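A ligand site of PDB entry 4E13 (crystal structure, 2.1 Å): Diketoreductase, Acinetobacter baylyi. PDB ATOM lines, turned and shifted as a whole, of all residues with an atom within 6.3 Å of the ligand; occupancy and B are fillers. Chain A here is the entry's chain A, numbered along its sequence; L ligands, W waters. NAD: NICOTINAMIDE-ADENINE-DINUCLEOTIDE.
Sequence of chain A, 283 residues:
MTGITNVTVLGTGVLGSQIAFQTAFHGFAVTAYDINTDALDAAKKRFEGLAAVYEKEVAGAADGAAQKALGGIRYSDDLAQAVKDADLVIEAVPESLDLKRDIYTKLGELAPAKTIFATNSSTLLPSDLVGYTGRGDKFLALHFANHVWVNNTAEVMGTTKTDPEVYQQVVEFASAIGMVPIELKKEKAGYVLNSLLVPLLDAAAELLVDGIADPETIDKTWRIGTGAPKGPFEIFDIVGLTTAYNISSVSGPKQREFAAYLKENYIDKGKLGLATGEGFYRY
An oxygen (O3B) of the ligand is in hydrogen-bond range of the backbone NH of Thr 12 (2.7 Å).
N of Ser 122 sits at hydrogen-bond distance from O2D of the ligand, 2.8 Å away.
The backbone NH of Val 14 sits at hydrogen-bond distance from an oxygen (O3) of the ligand (3.0 Å).
NZ of Lys 100 is in hydrogen-bond range of O3D of the ligand (3.2 Å).
The backbone NH (N) of Gly 13 sits at hydrogen-bond distance from an oxygen (O3B) of the ligand (3.1 Å).
The side-chain hydroxyl (OG1) of Thr 12 is in hydrogen-bond range of an oxygen (O3B) of the ligand (3.4 Å).
The side-chain amide nitrogen (ND2) of Asn 120 sits at hydrogen-bond distance from an oxygen (O4D) of the ligand (3.1 Å).
An oxygen (O2N) of the ligand sits at hydrogen-bond distance from the backbone NH (N) of Leu 15 (2.6 Å).
O2D of the ligand sits at hydrogen-bond distance from OG of Ser 122, at 2.9 Å.
The side-chain carboxylate (OD2) of Asp 34 lies within hydrogen-bond range of an oxygen (O3B) of the ligand, 2.6 Å away.
OE1 of Glu 95 is in hydrogen-bond range of O3D of the ligand (2.7 Å).
The backbone NH (N) of Gly 11 sits at hydrogen-bond distance from the backbone carbonyl oxygen (O) of Tyr 33, 2.7 Å away.
The backbone NH (N) of Ser 121 lies within hydrogen-bond range of the side-chain hydroxyl (OG1) of Thr 119 (3.1 Å).
The side-chain carboxylate (OE2) of Glu 95 is in hydrogen-bond range of the backbone NH (N) of Ser 122 (3.5 Å).
The backbone NH of Asn 120 sits at hydrogen-bond distance from the backbone carbonyl oxygen of Glu 91 (2.9 Å).
The side-chain carboxylate (OE2) of Glu 91 lies within hydrogen-bond range of the backbone NH (N) of Val 93.
The backbone carbonyl oxygen of Pro 94 lies within hydrogen-bond range of the side-chain amino group of Lys 100.
The backbone NH of Val 93 sits at hydrogen-bond distance from the backbone carbonyl oxygen of Leu 10.
The side-chain carboxylate of Asp 34 sits at hydrogen-bond distance from the side-chain hydroxyl of Thr 12 (2.6 Å).
Gly 11 touches the ligand (C to O3B, 3.6 Å).
Tyr 33 touches the ligand.
Ile 35 touches the ligand.
Ala 92 touches the ligand (O to C4B, 3.8 Å).
Val 93 touches the ligand.
CD of Pro 94 touches O4B of the ligand, at 3.4 Å.
CD2 of Leu 99 touches C6A of the ligand (3.4 Å).
Ile 103 touches the ligand.
Ser 121 touches the ligand (CA to O3D, 3.1 Å).
His 143 touches the ligand.
O of Phe 144 touches C5N of the ligand, 3.3 Å away.
CB of Asn 146 touches O7N of the ligand, 3.96 Å away.
Hydrophobic or aromatic side chains that line the ligand: Val 14, Leu 15, Tyr 33, Ile 35, Val 93, Pro 94, Leu 99, Ile 103 and His 143.
Within 4 Å of the ligand: Gly 11, Thr 12, Gly 13, Val 14, Leu 15, Tyr 33, Asp 34, Ile 35, Ala 92, Val 93, Pro 94, Glu 95, Leu 99, Lys 100, Ile 103, Asn 120, Ser 121, Ser 122, His 143, Phe 144 and Asn 146.
The nearest printed residue that does not touch the ligand is Gly 16 (4.4 Å).
Water W2 lies within hydrogen-bond range of N of Gly 13 (2.8 Å), N of Gly 16 (2.9 Å), O of Ala 92 (3.0 Å) and O3 of the ligand (3.2 Å).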
ATOM      1  N   LEU A  10     -24.595  15.633   5.288  1.00  0.00           N
ATOM      2  CA  LEU A  10     -23.700  15.460   4.151  1.00  0.00           C
ATOM      3  C   LEU A  10     -23.103  16.795   3.768  1.00  0.00           C
ATOM      4  O   LEU A  10     -23.793  17.677   3.247  1.00  0.00           O
ATOM      5  CB  LEU A  10     -24.455  14.894   2.946  1.00  0.00           C
ATOM      6  CG  LEU A  10     -25.261  13.615   3.174  1.00  0.00           C
ATOM      7  CD1 LEU A  10     -25.811  13.129   1.835  1.00  0.00           C
ATOM      8  CD2 LEU A  10     -24.379  12.535   3.812  1.00  0.00           C
ATOM      9  N   GLY A  11     -21.827  16.960   4.040  1.00  0.00           N
ATOM     10  CA  GLY A  11     -21.229  18.258   3.825  1.00  0.00           C
ATOM     11  C   GLY A  11     -21.025  18.984   5.135  1.00  0.00           C
ATOM     12  O   GLY A  11     -21.902  18.984   6.002  1.00  0.00           O
ATOM     13  N   THR A  12     -19.866  19.601   5.292  1.00  0.00           N
ATOM     14  CA  THR A  12     -19.507  20.251   6.535  1.00  0.00           C
ATOM     15  C   THR A  12     -19.076  21.663   6.237  1.00  0.00           C
ATOM     16  O   THR A  12     -18.248  22.254   6.949  1.00  0.00           O
ATOM     17  CB  THR A  12     -18.366  19.492   7.224  1.00  0.00           C
ATOM     18  OG1 THR A  12     -17.203  19.543   6.385  1.00  0.00           O
ATOM     19  CG2 THR A  12     -18.765  18.042   7.455  1.00  0.00           C
ATOM     20  N   GLY A  13     -19.626  22.205   5.165  1.00  0.00           N
ATOM     21  CA  GLY A  13     -19.330  23.585   4.805  1.00  0.00           C
ATOM     22  C   GLY A  13     -20.045  24.588   5.688  1.00  0.00           C
ATOM     23  O   GLY A  13     -20.368  24.305   6.848  1.00  0.00           O
ATOM     24  N   VAL A  14     -20.286  25.763   5.127  1.00  0.00           N
ATOM     25  CA  VAL A  14     -20.880  26.849   5.894  1.00  0.00           C
ATOM     26  C   VAL A  14     -22.168  26.442   6.581  1.00  0.00           C
ATOM     27  O   VAL A  14     -22.319  26.650   7.788  1.00  0.00           O
ATOM     28  CB  VAL A  14     -21.128  28.089   5.034  1.00  0.00           C
ATOM     29  CG1 VAL A  14     -21.783  29.191   5.878  1.00  0.00           C
ATOM     30  CG2 VAL A  14     -19.801  28.563   4.442  1.00  0.00           C
ATOM     31  N   LEU A  15     -23.108  25.868   5.835  1.00  0.00           N
ATOM     32  CA  LEU A  15     -24.360  25.462   6.446  1.00  0.00           C
ATOM     33  C   LEU A  15     -24.359  24.042   6.990  1.00  0.00           C
ATOM     34  O   LEU A  15     -25.085  23.756   7.947  1.00  0.00           O
ATOM     35  CB  LEU A  15     -25.562  25.684   5.541  1.00  0.00           C
ATOM     36  CG  LEU A  15     -26.303  26.967   5.894  1.00  0.00           C
ATOM     37  CD1 LEU A  15     -25.529  28.191   5.460  1.00  0.00           C
ATOM     38  CD2 LEU A  15     -27.659  26.924   5.242  1.00  0.00           C
ATOM     39  N   GLY A  16     -23.571  23.169   6.381  1.00  0.00           N
ATOM     40  CA  GLY A  16     -23.477  21.809   6.894  1.00  0.00           C
ATOM     41  C   GLY A  16     -22.949  21.738   8.309  1.00  0.00           C
ATOM     42  O   GLY A  16     -23.492  21.009   9.155  1.00  0.00           O
ATOM     43  N   TYR A  33     -20.555  13.960   7.480  1.00  0.00           N
ATOM     44  CA  TYR A  33     -19.935  13.309   6.325  1.00  0.00           C
ATOM     45  C   TYR A  33     -19.331  14.311   5.359  1.00  0.00           C
ATOM     46  O   TYR A  33     -19.940  15.333   5.032  1.00  0.00           O
ATOM     47  CB  TYR A  33     -20.954  12.472   5.573  1.00  0.00           C
ATOM     48  CG  TYR A  33     -20.403  12.002   4.242  1.00  0.00           C
ATOM     49  CD1 TYR A  33     -19.660  10.818   4.144  1.00  0.00           C
ATOM     50  CD2 TYR A  33     -20.622  12.746   3.087  1.00  0.00           C
ATOM     51  CE1 TYR A  33     -19.149  10.392   2.912  1.00  0.00           C
ATOM     52  CE2 TYR A  33     -20.119  12.327   1.855  1.00  0.00           C
ATOM     53  CZ  TYR A  33     -19.382  11.167   1.772  1.00  0.00           C
ATOM     54  OH  TYR A  33     -18.899  10.770   0.553  1.00  0.00           O
ATOM     55  N   ASP A  34     -18.132  13.997   4.873  1.00  0.00           N
ATOM     56  CA  ASP A  34     -17.499  14.818   3.846  1.00  0.00           C
ATOM     57  C   ASP A  34     -16.569  13.923   3.015  1.00  0.00           C
ATOM     58  O   ASP A  34     -16.393  12.750   3.348  1.00  0.00           O
ATOM     59  CB  ASP A  34     -16.747  15.987   4.480  1.00  0.00           C
ATOM     60  CG  ASP A  34     -16.745  17.231   3.600  1.00  0.00           C
ATOM     61  OD1 ASP A  34     -16.849  17.117   2.365  1.00  0.00           O
ATOM     62  OD2 ASP A  34     -16.649  18.334   4.172  1.00  0.00           O
ATOM     63  N   ILE A  35     -15.970  14.479   1.969  1.00  0.00           N
ATOM     64  CA  ILE A  35     -15.355  13.632   0.931  1.00  0.00           C
ATOM     65  C   ILE A  35     -14.043  12.944   1.300  1.00  0.00           C
ATOM     66  O   ILE A  35     -13.764  11.845   0.812  1.00  0.00           O
ATOM     67  CB  ILE A  35     -15.210  14.370  -0.406  1.00  0.00           C
ATOM     68  CG1 ILE A  35     -14.247  15.550  -0.257  1.00  0.00           C
ATOM     69  CG2 ILE A  35     -16.572  14.804  -0.899  1.00  0.00           C
ATOM     70  CD1 ILE A  35     -14.043  16.317  -1.545  1.00  0.00           C
ATOM     71  N   ALA A  39     -11.079  17.194   4.192  1.00  0.00           N
ATOM     72  CA  ALA A  39     -12.343  17.919   4.362  1.00  0.00           C
ATOM     73  C   ALA A  39     -12.832  17.742   5.813  1.00  0.00           C
ATOM     74  O   ALA A  39     -13.392  18.656   6.418  1.00  0.00           O
ATOM     75  CB  ALA A  39     -13.380  17.402   3.374  1.00  0.00           C
ATOM     76  N   ARG A  46     -14.162  24.010  11.828  1.00  0.00           N
ATOM     77  CA  ARG A  46     -15.409  24.761  11.892  1.00  0.00           C
ATOM     78  C   ARG A  46     -16.177  24.443  13.158  1.00  0.00           C
ATOM     79  O   ARG A  46     -16.708  25.346  13.806  1.00  0.00           O
ATOM     80  CB  ARG A  46     -16.319  24.473  10.700  1.00  0.00           C
ATOM     81  CG  ARG A  46     -15.748  24.929   9.384  1.00  0.00           C
ATOM     82  CD  ARG A  46     -16.709  24.656   8.249  1.00  0.00           C
ATOM     83  NE  ARG A  46     -16.075  24.959   6.978  1.00  0.00           N
ATOM     84  CZ  ARG A  46     -15.306  24.094   6.316  1.00  0.00           C
ATOM     85  NH1 ARG A  46     -15.110  22.877   6.797  1.00  0.00           N
ATOM     86  NH2 ARG A  46     -14.746  24.446   5.161  1.00  0.00           N
ATOM     87  N   GLU A  91     -28.809  16.968   3.797  1.00  0.00           N
ATOM     88  CA  GLU A  91     -27.892  17.129   2.695  1.00  0.00           C
ATOM     89  C   GLU A  91     -27.602  18.599   2.451  1.00  0.00           C
ATOM     90  O   GLU A  91     -28.504  19.390   2.143  1.00  0.00           O
ATOM     91  CB  GLU A  91     -28.486  16.444   1.456  1.00  0.00           C
ATOM     92  CG  GLU A  91     -27.687  16.652   0.178  1.00  0.00           C
ATOM     93  CD  GLU A  91     -27.954  17.996  -0.471  1.00  0.00           C
ATOM     94  OE1 GLU A  91     -29.118  18.226  -0.877  1.00  0.00           O
ATOM     95  OE2 GLU A  91     -27.018  18.824  -0.580  1.00  0.00           O
ATOM     96  N   ALA A  92     -26.346  18.976   2.647  1.00  0.00           N
ATOM     97  CA  ALA A  92     -25.891  20.336   2.372  1.00  0.00           C
ATOM     98  C   ALA A  92     -24.610  20.242   1.548  1.00  0.00           C
ATOM     99  O   ALA A  92     -23.577  20.801   1.941  1.00  0.00           O
ATOM    100  CB  ALA A  92     -25.630  21.087   3.676  1.00  0.00           C
ATOM    101  N   VAL A  93     -24.678  19.530   0.420  1.00  0.00           N
ATOM    102  CA  VAL A  93     -23.549  19.469  -0.504  1.00  0.00           C
ATOM    103  C   VAL A  93     -23.611  20.710  -1.385  1.00  0.00           C
ATOM    104  O   VAL A  93     -24.622  21.412  -1.378  1.00  0.00           O
ATOM    105  CB  VAL A  93     -23.557  18.172  -1.360  1.00  0.00           C
ATOM    106  CG1 VAL A  93     -23.563  16.939  -0.468  1.00  0.00           C
ATOM    107  CG2 VAL A  93     -24.737  18.138  -2.315  1.00  0.00           C
ATOM    108  N   PRO A  94     -22.532  21.001  -2.147  1.00  0.00           N
ATOM    109  CA  PRO A  94     -22.512  22.185  -3.008  1.00  0.00           C
ATOM    110  C   PRO A  94     -23.735  22.310  -3.888  1.00  0.00           C
ATOM    111  O   PRO A  94     -24.351  21.304  -4.251  1.00  0.00           O
ATOM    112  CB  PRO A  94     -21.222  22.019  -3.828  1.00  0.00           C
ATOM    113  CG  PRO A  94     -20.357  21.167  -2.968  1.00  0.00           C
ATOM    114  CD  PRO A  94     -21.293  20.208  -2.296  1.00  0.00           C
ATOM    115  N   GLU A  95     -24.093  23.541  -4.226  1.00  0.00           N
ATOM    116  CA  GLU A  95     -25.285  23.791  -5.018  1.00  0.00           C
ATOM    117  C   GLU A  95     -24.940  23.482  -6.478  1.00  0.00           C
ATOM    118  O   GLU A  95     -24.514  24.355  -7.234  1.00  0.00           O
ATOM    119  CB  GLU A  95     -25.734  25.241  -4.856  1.00  0.00           C
ATOM    120  CG  GLU A  95     -27.130  25.530  -5.380  1.00  0.00           C
ATOM    121  CD  GLU A  95     -28.207  24.800  -4.592  1.00  0.00           C
ATOM    122  OE1 GLU A  95     -27.854  23.908  -3.795  1.00  0.00           O
ATOM    123  OE2 GLU A  95     -29.399  25.122  -4.771  1.00  0.00           O
ATOM    124  N   LEU A  99     -23.739  17.260  -8.860  1.00  0.00           N
ATOM    125  CA  LEU A  99     -23.114  16.766  -7.648  1.00  0.00           C
ATOM    126  C   LEU A  99     -24.165  16.237  -6.649  1.00  0.00           C
ATOM    127  O   LEU A  99     -23.892  15.304  -5.896  1.00  0.00           O
ATOM    128  CB  LEU A  99     -22.253  17.881  -7.051  1.00  0.00           C
ATOM    129  CG  LEU A  99     -21.226  17.567  -5.968  1.00  0.00           C
ATOM    130  CD1 LEU A  99     -20.355  18.789  -5.719  1.00  0.00           C
ATOM    131  CD2 LEU A  99     -21.902  17.088  -4.696  1.00  0.00           C
ATOM    132  N   LYS A 100     -25.368  16.828  -6.658  1.00  0.00           N
ATOM    133  CA  LYS A 100     -26.461  16.347  -5.811  1.00  0.00           C
ATOM    134  C   LYS A 100     -27.126  15.109  -6.395  1.00  0.00           C
ATOM    135  O   LYS A 100     -27.634  14.244  -5.671  1.00  0.00           O
ATOM    136  CB  LYS A 100     -27.519  17.453  -5.575  1.00  0.00           C
ATOM    137  CG  LYS A 100     -27.104  18.560  -4.594  1.00  0.00           C
ATOM    138  CD  LYS A 100     -28.217  19.591  -4.396  1.00  0.00           C
ATOM    139  CE  LYS A 100     -28.017  20.431  -3.142  1.00  0.00           C
ATOM    140  NZ  LYS A 100     -26.669  21.037  -3.051  1.00  0.00           N
ATOM    141  N   ASP A 102     -25.550  12.797  -8.181  1.00  0.00           N
ATOM    142  CA  ASP A 102     -24.596  11.771  -7.799  1.00  0.00           C
ATOM    143  C   ASP A 102     -24.870  11.312  -6.362  1.00  0.00           C
ATOM    144  O   ASP A 102     -25.064  10.124  -6.094  1.00  0.00           O
ATOM    145  CB  ASP A 102     -23.186  12.332  -7.917  1.00  0.00           C
ATOM    146  CG  ASP A 102     -22.107  11.341  -7.526  1.00  0.00           C
ATOM    147  OD1 ASP A 102     -22.450  10.282  -6.959  1.00  0.00           O
ATOM    148  OD2 ASP A 102     -20.924  11.627  -7.782  1.00  0.00           O
ATOM    149  N   ILE A 103     -24.890  12.282  -5.445  1.00  0.00           N
ATOM    150  CA  ILE A 103     -25.159  12.034  -4.028  1.00  0.00           C
ATOM    151  C   ILE A 103     -26.413  11.209  -3.751  1.00  0.00           C
ATOM    152  O   ILE A 103     -26.329  10.172  -3.077  1.00  0.00           O
ATOM    153  CB  ILE A 103     -25.257  13.358  -3.245  1.00  0.00           C
ATOM    154  CG1 ILE A 103     -23.870  13.789  -2.794  1.00  0.00           C
ATOM    155  CG2 ILE A 103     -26.224  13.228  -2.091  1.00  0.00           C
ATOM    156  CD1 ILE A 103     -23.247  12.839  -1.780  1.00  0.00           C
ATOM    157  N   THR A 119     -33.016  17.860   1.947  1.00  0.00           N
ATOM    158  CA  THR A 119     -32.062  18.743   1.270  1.00  0.00           C
ATOM    159  C   THR A 119     -32.138  20.168   1.842  1.00  0.00           C
ATOM    160  O   THR A 119     -33.225  20.656   2.159  1.00  0.00           O
ATOM    161  CB  THR A 119     -32.350  18.839  -0.236  1.00  0.00           C
ATOM    162  OG1 THR A 119     -31.436  19.749  -0.839  1.00  0.00           O
ATOM    163  CG2 THR A 119     -33.778  19.314  -0.468  1.00  0.00           C
ATOM    164  N   ASN A 120     -30.992  20.820   1.932  1.00  0.00           N
ATOM    165  CA  ASN A 120     -30.904  22.201   2.436  1.00  0.00           C
ATOM    166  C   ASN A 120     -30.792  23.162   1.264  1.00  0.00           C
ATOM    167  O   ASN A 120     -30.492  24.349   1.452  1.00  0.00           O
ATOM    168  CB  ASN A 120     -29.657  22.364   3.298  1.00  0.00           C
ATOM    169  CG  ASN A 120     -29.557  23.760   3.912  1.00  0.00           C
ATOM    170  OD1 ASN A 120     -30.532  24.277   4.454  1.00  0.00           O
ATOM    171  ND2 ASN A 120     -28.375  24.363   3.819  1.00  0.00           N
ATOM    172  N   SER A 121     -31.015  22.646   0.055  1.00  0.00           N
ATOM    173  CA  SER A 121     -30.753  23.406  -1.153  1.00  0.00           C
ATOM    174  C   SER A 121     -31.513  24.741  -1.218  1.00  0.00           C
ATOM    175  O   SER A 121     -32.689  24.817  -0.871  1.00  0.00           O
ATOM    176  CB  SER A 121     -31.086  22.570  -2.397  1.00  0.00           C
ATOM    177  OG  SER A 121     -30.752  23.274  -3.565  1.00  0.00           O
ATOM    178  N   SER A 122     -30.824  25.779  -1.649  1.00  0.00           N
ATOM    179  CA  SER A 122     -31.440  27.078  -1.867  1.00  0.00           C
ATOM    180  C   SER A 122     -32.222  27.087  -3.173  1.00  0.00           C
ATOM    181  O   SER A 122     -33.424  27.341  -3.183  1.00  0.00           O
ATOM    182  CB  SER A 122     -30.382  28.188  -1.896  1.00  0.00           C
ATOM    183  OG  SER A 122     -29.712  28.297  -0.652  1.00  0.00           O
ATOM    184  N   THR A 123     -31.516  26.807  -4.274  1.00  0.00           N
ATOM    185  CA  THR A 123     -32.070  26.994  -5.602  1.00  0.00           C
ATOM    186  C   THR A 123     -32.631  25.713  -6.243  1.00  0.00           C
ATOM    187  O   THR A 123     -33.638  25.758  -6.951  1.00  0.00           O
ATOM    188  CB  THR A 123     -31.031  27.624  -6.537  1.00  0.00           C
ATOM    189  OG1 THR A 123     -29.883  26.772  -6.622  1.00  0.00           O
ATOM    190  CG2 THR A 123     -30.592  28.975  -5.982  1.00  0.00           C
ATOM    191  N   LEU A 124     -31.985  24.575  -5.992  1.00  0.00           N
ATOM    192  CA  LEU A 124     -32.456  23.314  -6.550  1.00  0.00           C
ATOM    193  C   LEU A 124     -33.726  22.815  -5.861  1.00  0.00           C
ATOM    194  O   LEU A 124     -33.729  22.528  -4.659  1.00  0.00           O
ATOM    195  CB  LEU A 124     -31.353  22.246  -6.487  1.00  0.00           C
ATOM    196  CG  LEU A 124     -30.136  22.592  -7.358  1.00  0.00           C
ATOM    197  CD1 LEU A 124     -28.991  21.612  -7.163  1.00  0.00           C
ATOM    198  CD2 LEU A 124     -30.552  22.650  -8.822  1.00  0.00           C
ATOM    199  N   HIS A 143     -34.842  23.723   4.930  1.00  0.00           N
ATOM    200  CA  HIS A 143     -33.983  24.823   4.521  1.00  0.00           C
ATOM    201  C   HIS A 143     -33.664  25.777   5.687  1.00  0.00           C
ATOM    202  O   HIS A 143     -34.573  26.350   6.295  1.00  0.00           O
ATOM    203  CB  HIS A 143     -34.665  25.577   3.385  1.00  0.00           C
ATOM    204  CG  HIS A 143     -33.825  26.656   2.790  1.00  0.00           C
ATOM    205  ND1 HIS A 143     -34.161  27.993   2.858  1.00  0.00           N
ATOM    206  CD2 HIS A 143     -32.652  26.600   2.114  1.00  0.00           C
ATOM    207  CE1 HIS A 143     -33.227  28.709   2.251  1.00  0.00           C
ATOM    208  NE2 HIS A 143     -32.300  27.885   1.793  1.00  0.00           N
ATOM    209  N   PHE A 144     -32.374  25.927   5.969  1.00  0.00           N
ATOM    210  CA  PHE A 144     -31.896  26.743   7.085  1.00  0.00           C
ATOM    211  C   PHE A 144     -31.399  28.096   6.607  1.00  0.00           C
ATOM    212  O   PHE A 144     -31.210  28.314   5.398  1.00  0.00           O
ATOM    213  CB  PHE A 144     -30.747  26.028   7.817  1.00  0.00           C
ATOM    214  CG  PHE A 144     -31.170  24.754   8.495  1.00  0.00           C
ATOM    215  CD1 PHE A 144     -31.319  23.565   7.768  1.00  0.00           C
ATOM    216  CD2 PHE A 144     -31.414  24.728   9.857  1.00  0.00           C
ATOM    217  CE1 PHE A 144     -31.709  22.390   8.392  1.00  0.00           C
ATOM    218  CE2 PHE A 144     -31.800  23.558  10.494  1.00  0.00           C
ATOM    219  CZ  PHE A 144     -31.950  22.385   9.760  1.00  0.00           C
ATOM    220  N   ALA A 145     -31.161  28.994   7.558  1.00  0.00           N
ATOM    221  CA  ALA A 145     -30.598  30.298   7.255  1.00  0.00           C
ATOM    222  C   ALA A 145     -29.210  30.404   7.886  1.00  0.00           C
ATOM    223  O   ALA A 145     -28.958  29.859   8.961  1.00  0.00           O
ATOM    224  CB  ALA A 145     -31.495  31.397   7.787  1.00  0.00           C
ATOM    225  N   ASN A 146     -28.307  31.113   7.220  1.00  0.00           N
ATOM    226  CA  ASN A 146     -26.951  31.264   7.721  1.00  0.00           C
ATOM    227  C   ASN A 146     -26.987  31.894   9.135  1.00  0.00           C
ATOM    228  O   ASN A 146     -27.701  32.879   9.366  1.00  0.00           O
ATOM    229  CB  ASN A 146     -26.154  32.156   6.770  1.00  0.00           C
ATOM    230  CG  ASN A 146     -24.684  32.194   7.106  1.00  0.00           C
ATOM    231  OD1 ASN A 146     -24.172  31.287   7.768  1.00  0.00           O
ATOM    232  ND2 ASN A 146     -24.005  33.252   6.678  1.00  0.00           N
HETATM  233  PA  NAD L   1     -20.291  25.009   1.400  1.00  0.00           P
HETATM  234  O1A NAD L   1     -19.258  25.992   1.763  1.00  0.00           O
HETATM  235  O2A NAD L   1     -20.875  25.020   0.044  1.00  0.00           O
HETATM  236  O5B NAD L   1     -19.728  23.534   1.711  1.00  0.00           O
HETATM  237  C5B NAD L   1     -20.120  22.405   0.917  1.00  0.00           C
HETATM  238  C4B NAD L   1     -19.842  21.138   1.723  1.00  0.00           C
HETATM  239  O4B NAD L   1     -20.022  20.013   0.850  1.00  0.00           O
HETATM  240  C3B NAD L   1     -18.371  21.126   2.119  1.00  0.00           C
HETATM  241  O3B NAD L   1     -18.180  20.277   3.265  1.00  0.00           O
HETATM  242  C2B NAD L   1     -17.745  20.485   0.894  1.00  0.00           C
HETATM  243  O2B NAD L   1     -16.469  19.935   1.240  1.00  0.00           O
HETATM  244  C1B NAD L   1     -18.745  19.356   0.751  1.00  0.00           C
HETATM  245  N9A NAD L   1     -18.592  18.610  -0.515  1.00  0.00           N
HETATM  246  C8A NAD L   1     -17.955  19.015  -1.614  1.00  0.00           C
HETATM  247  N7A NAD L   1     -18.185  18.111  -2.566  1.00  0.00           N
HETATM  248  C5A NAD L   1     -18.935  17.140  -2.054  1.00  0.00           C
HETATM  249  C6A NAD L   1     -19.403  16.019  -2.577  1.00  0.00           C
HETATM  250  N6A NAD L   1     -18.869  15.657  -3.748  1.00  0.00           N
HETATM  251  N1A NAD L   1     -20.170  15.173  -1.881  1.00  0.00           N
HETATM  252  C2A NAD L   1     -20.475  15.472  -0.542  1.00  0.00           C
HETATM  253  N3A NAD L   1     -19.951  16.653  -0.016  1.00  0.00           N
HETATM  254  C4A NAD L   1     -19.202  17.459  -0.777  1.00  0.00           C
HETATM  255  O3  NAD L   1     -21.487  25.144   2.468  1.00  0.00           O
HETATM  256  PN  NAD L   1     -22.883  25.853   2.069  1.00  0.00           P
HETATM  257  O1N NAD L   1     -22.637  26.808   0.960  1.00  0.00           O
HETATM  258  O2N NAD L   1     -23.533  26.344   3.295  1.00  0.00           O
HETATM  259  O5D NAD L   1     -23.751  24.626   1.507  1.00  0.00           O
HETATM  260  C5D NAD L   1     -24.410  24.736   0.246  1.00  0.00           C
HETATM  261  C4D NAD L   1     -25.742  23.995   0.311  1.00  0.00           C
HETATM  262  O4D NAD L   1     -26.518  24.587   1.374  1.00  0.00           O
HETATM  263  C3D NAD L   1     -26.513  24.307  -0.959  1.00  0.00           C
HETATM  264  O3D NAD L   1     -27.642  23.442  -1.100  1.00  0.00           O
HETATM  265  C2D NAD L   1     -26.946  25.725  -0.637  1.00  0.00           C
HETATM  266  O2D NAD L   1     -28.026  26.114  -1.501  1.00  0.00           O
HETATM  267  C1D NAD L   1     -27.480  25.472   0.757  1.00  0.00           C
HETATM  268  N1N NAD L   1     -27.725  26.712   1.536  1.00  0.00           N
HETATM  269  C2N NAD L   1     -26.693  27.631   1.726  1.00  0.00           C
HETATM  270  C3N NAD L   1     -26.928  28.820   2.411  1.00  0.00           C
HETATM  271  C7N NAD L   1     -25.902  29.728   2.608  1.00  0.00           C
HETATM  272  O7N NAD L   1     -26.129  30.866   3.031  1.00  0.00           O
HETATM  273  N7N NAD L   1     -24.683  29.285   2.292  1.00  0.00           N
HETATM  274  C4N NAD L   1     -28.207  29.091   2.893  1.00  0.00           C
HETATM  275  C5N NAD L   1     -29.238  28.175   2.725  1.00  0.00           C
HETATM  276  C6N NAD L   1     -28.996  26.978   2.050  1.00  0.00           C
HETATM  277  O   HOH W   1     -29.174  32.040   4.479  1.00  0.00           O
HETATM  278  O   HOH W   2     -22.149  22.423   3.957  1.00  0.00           O
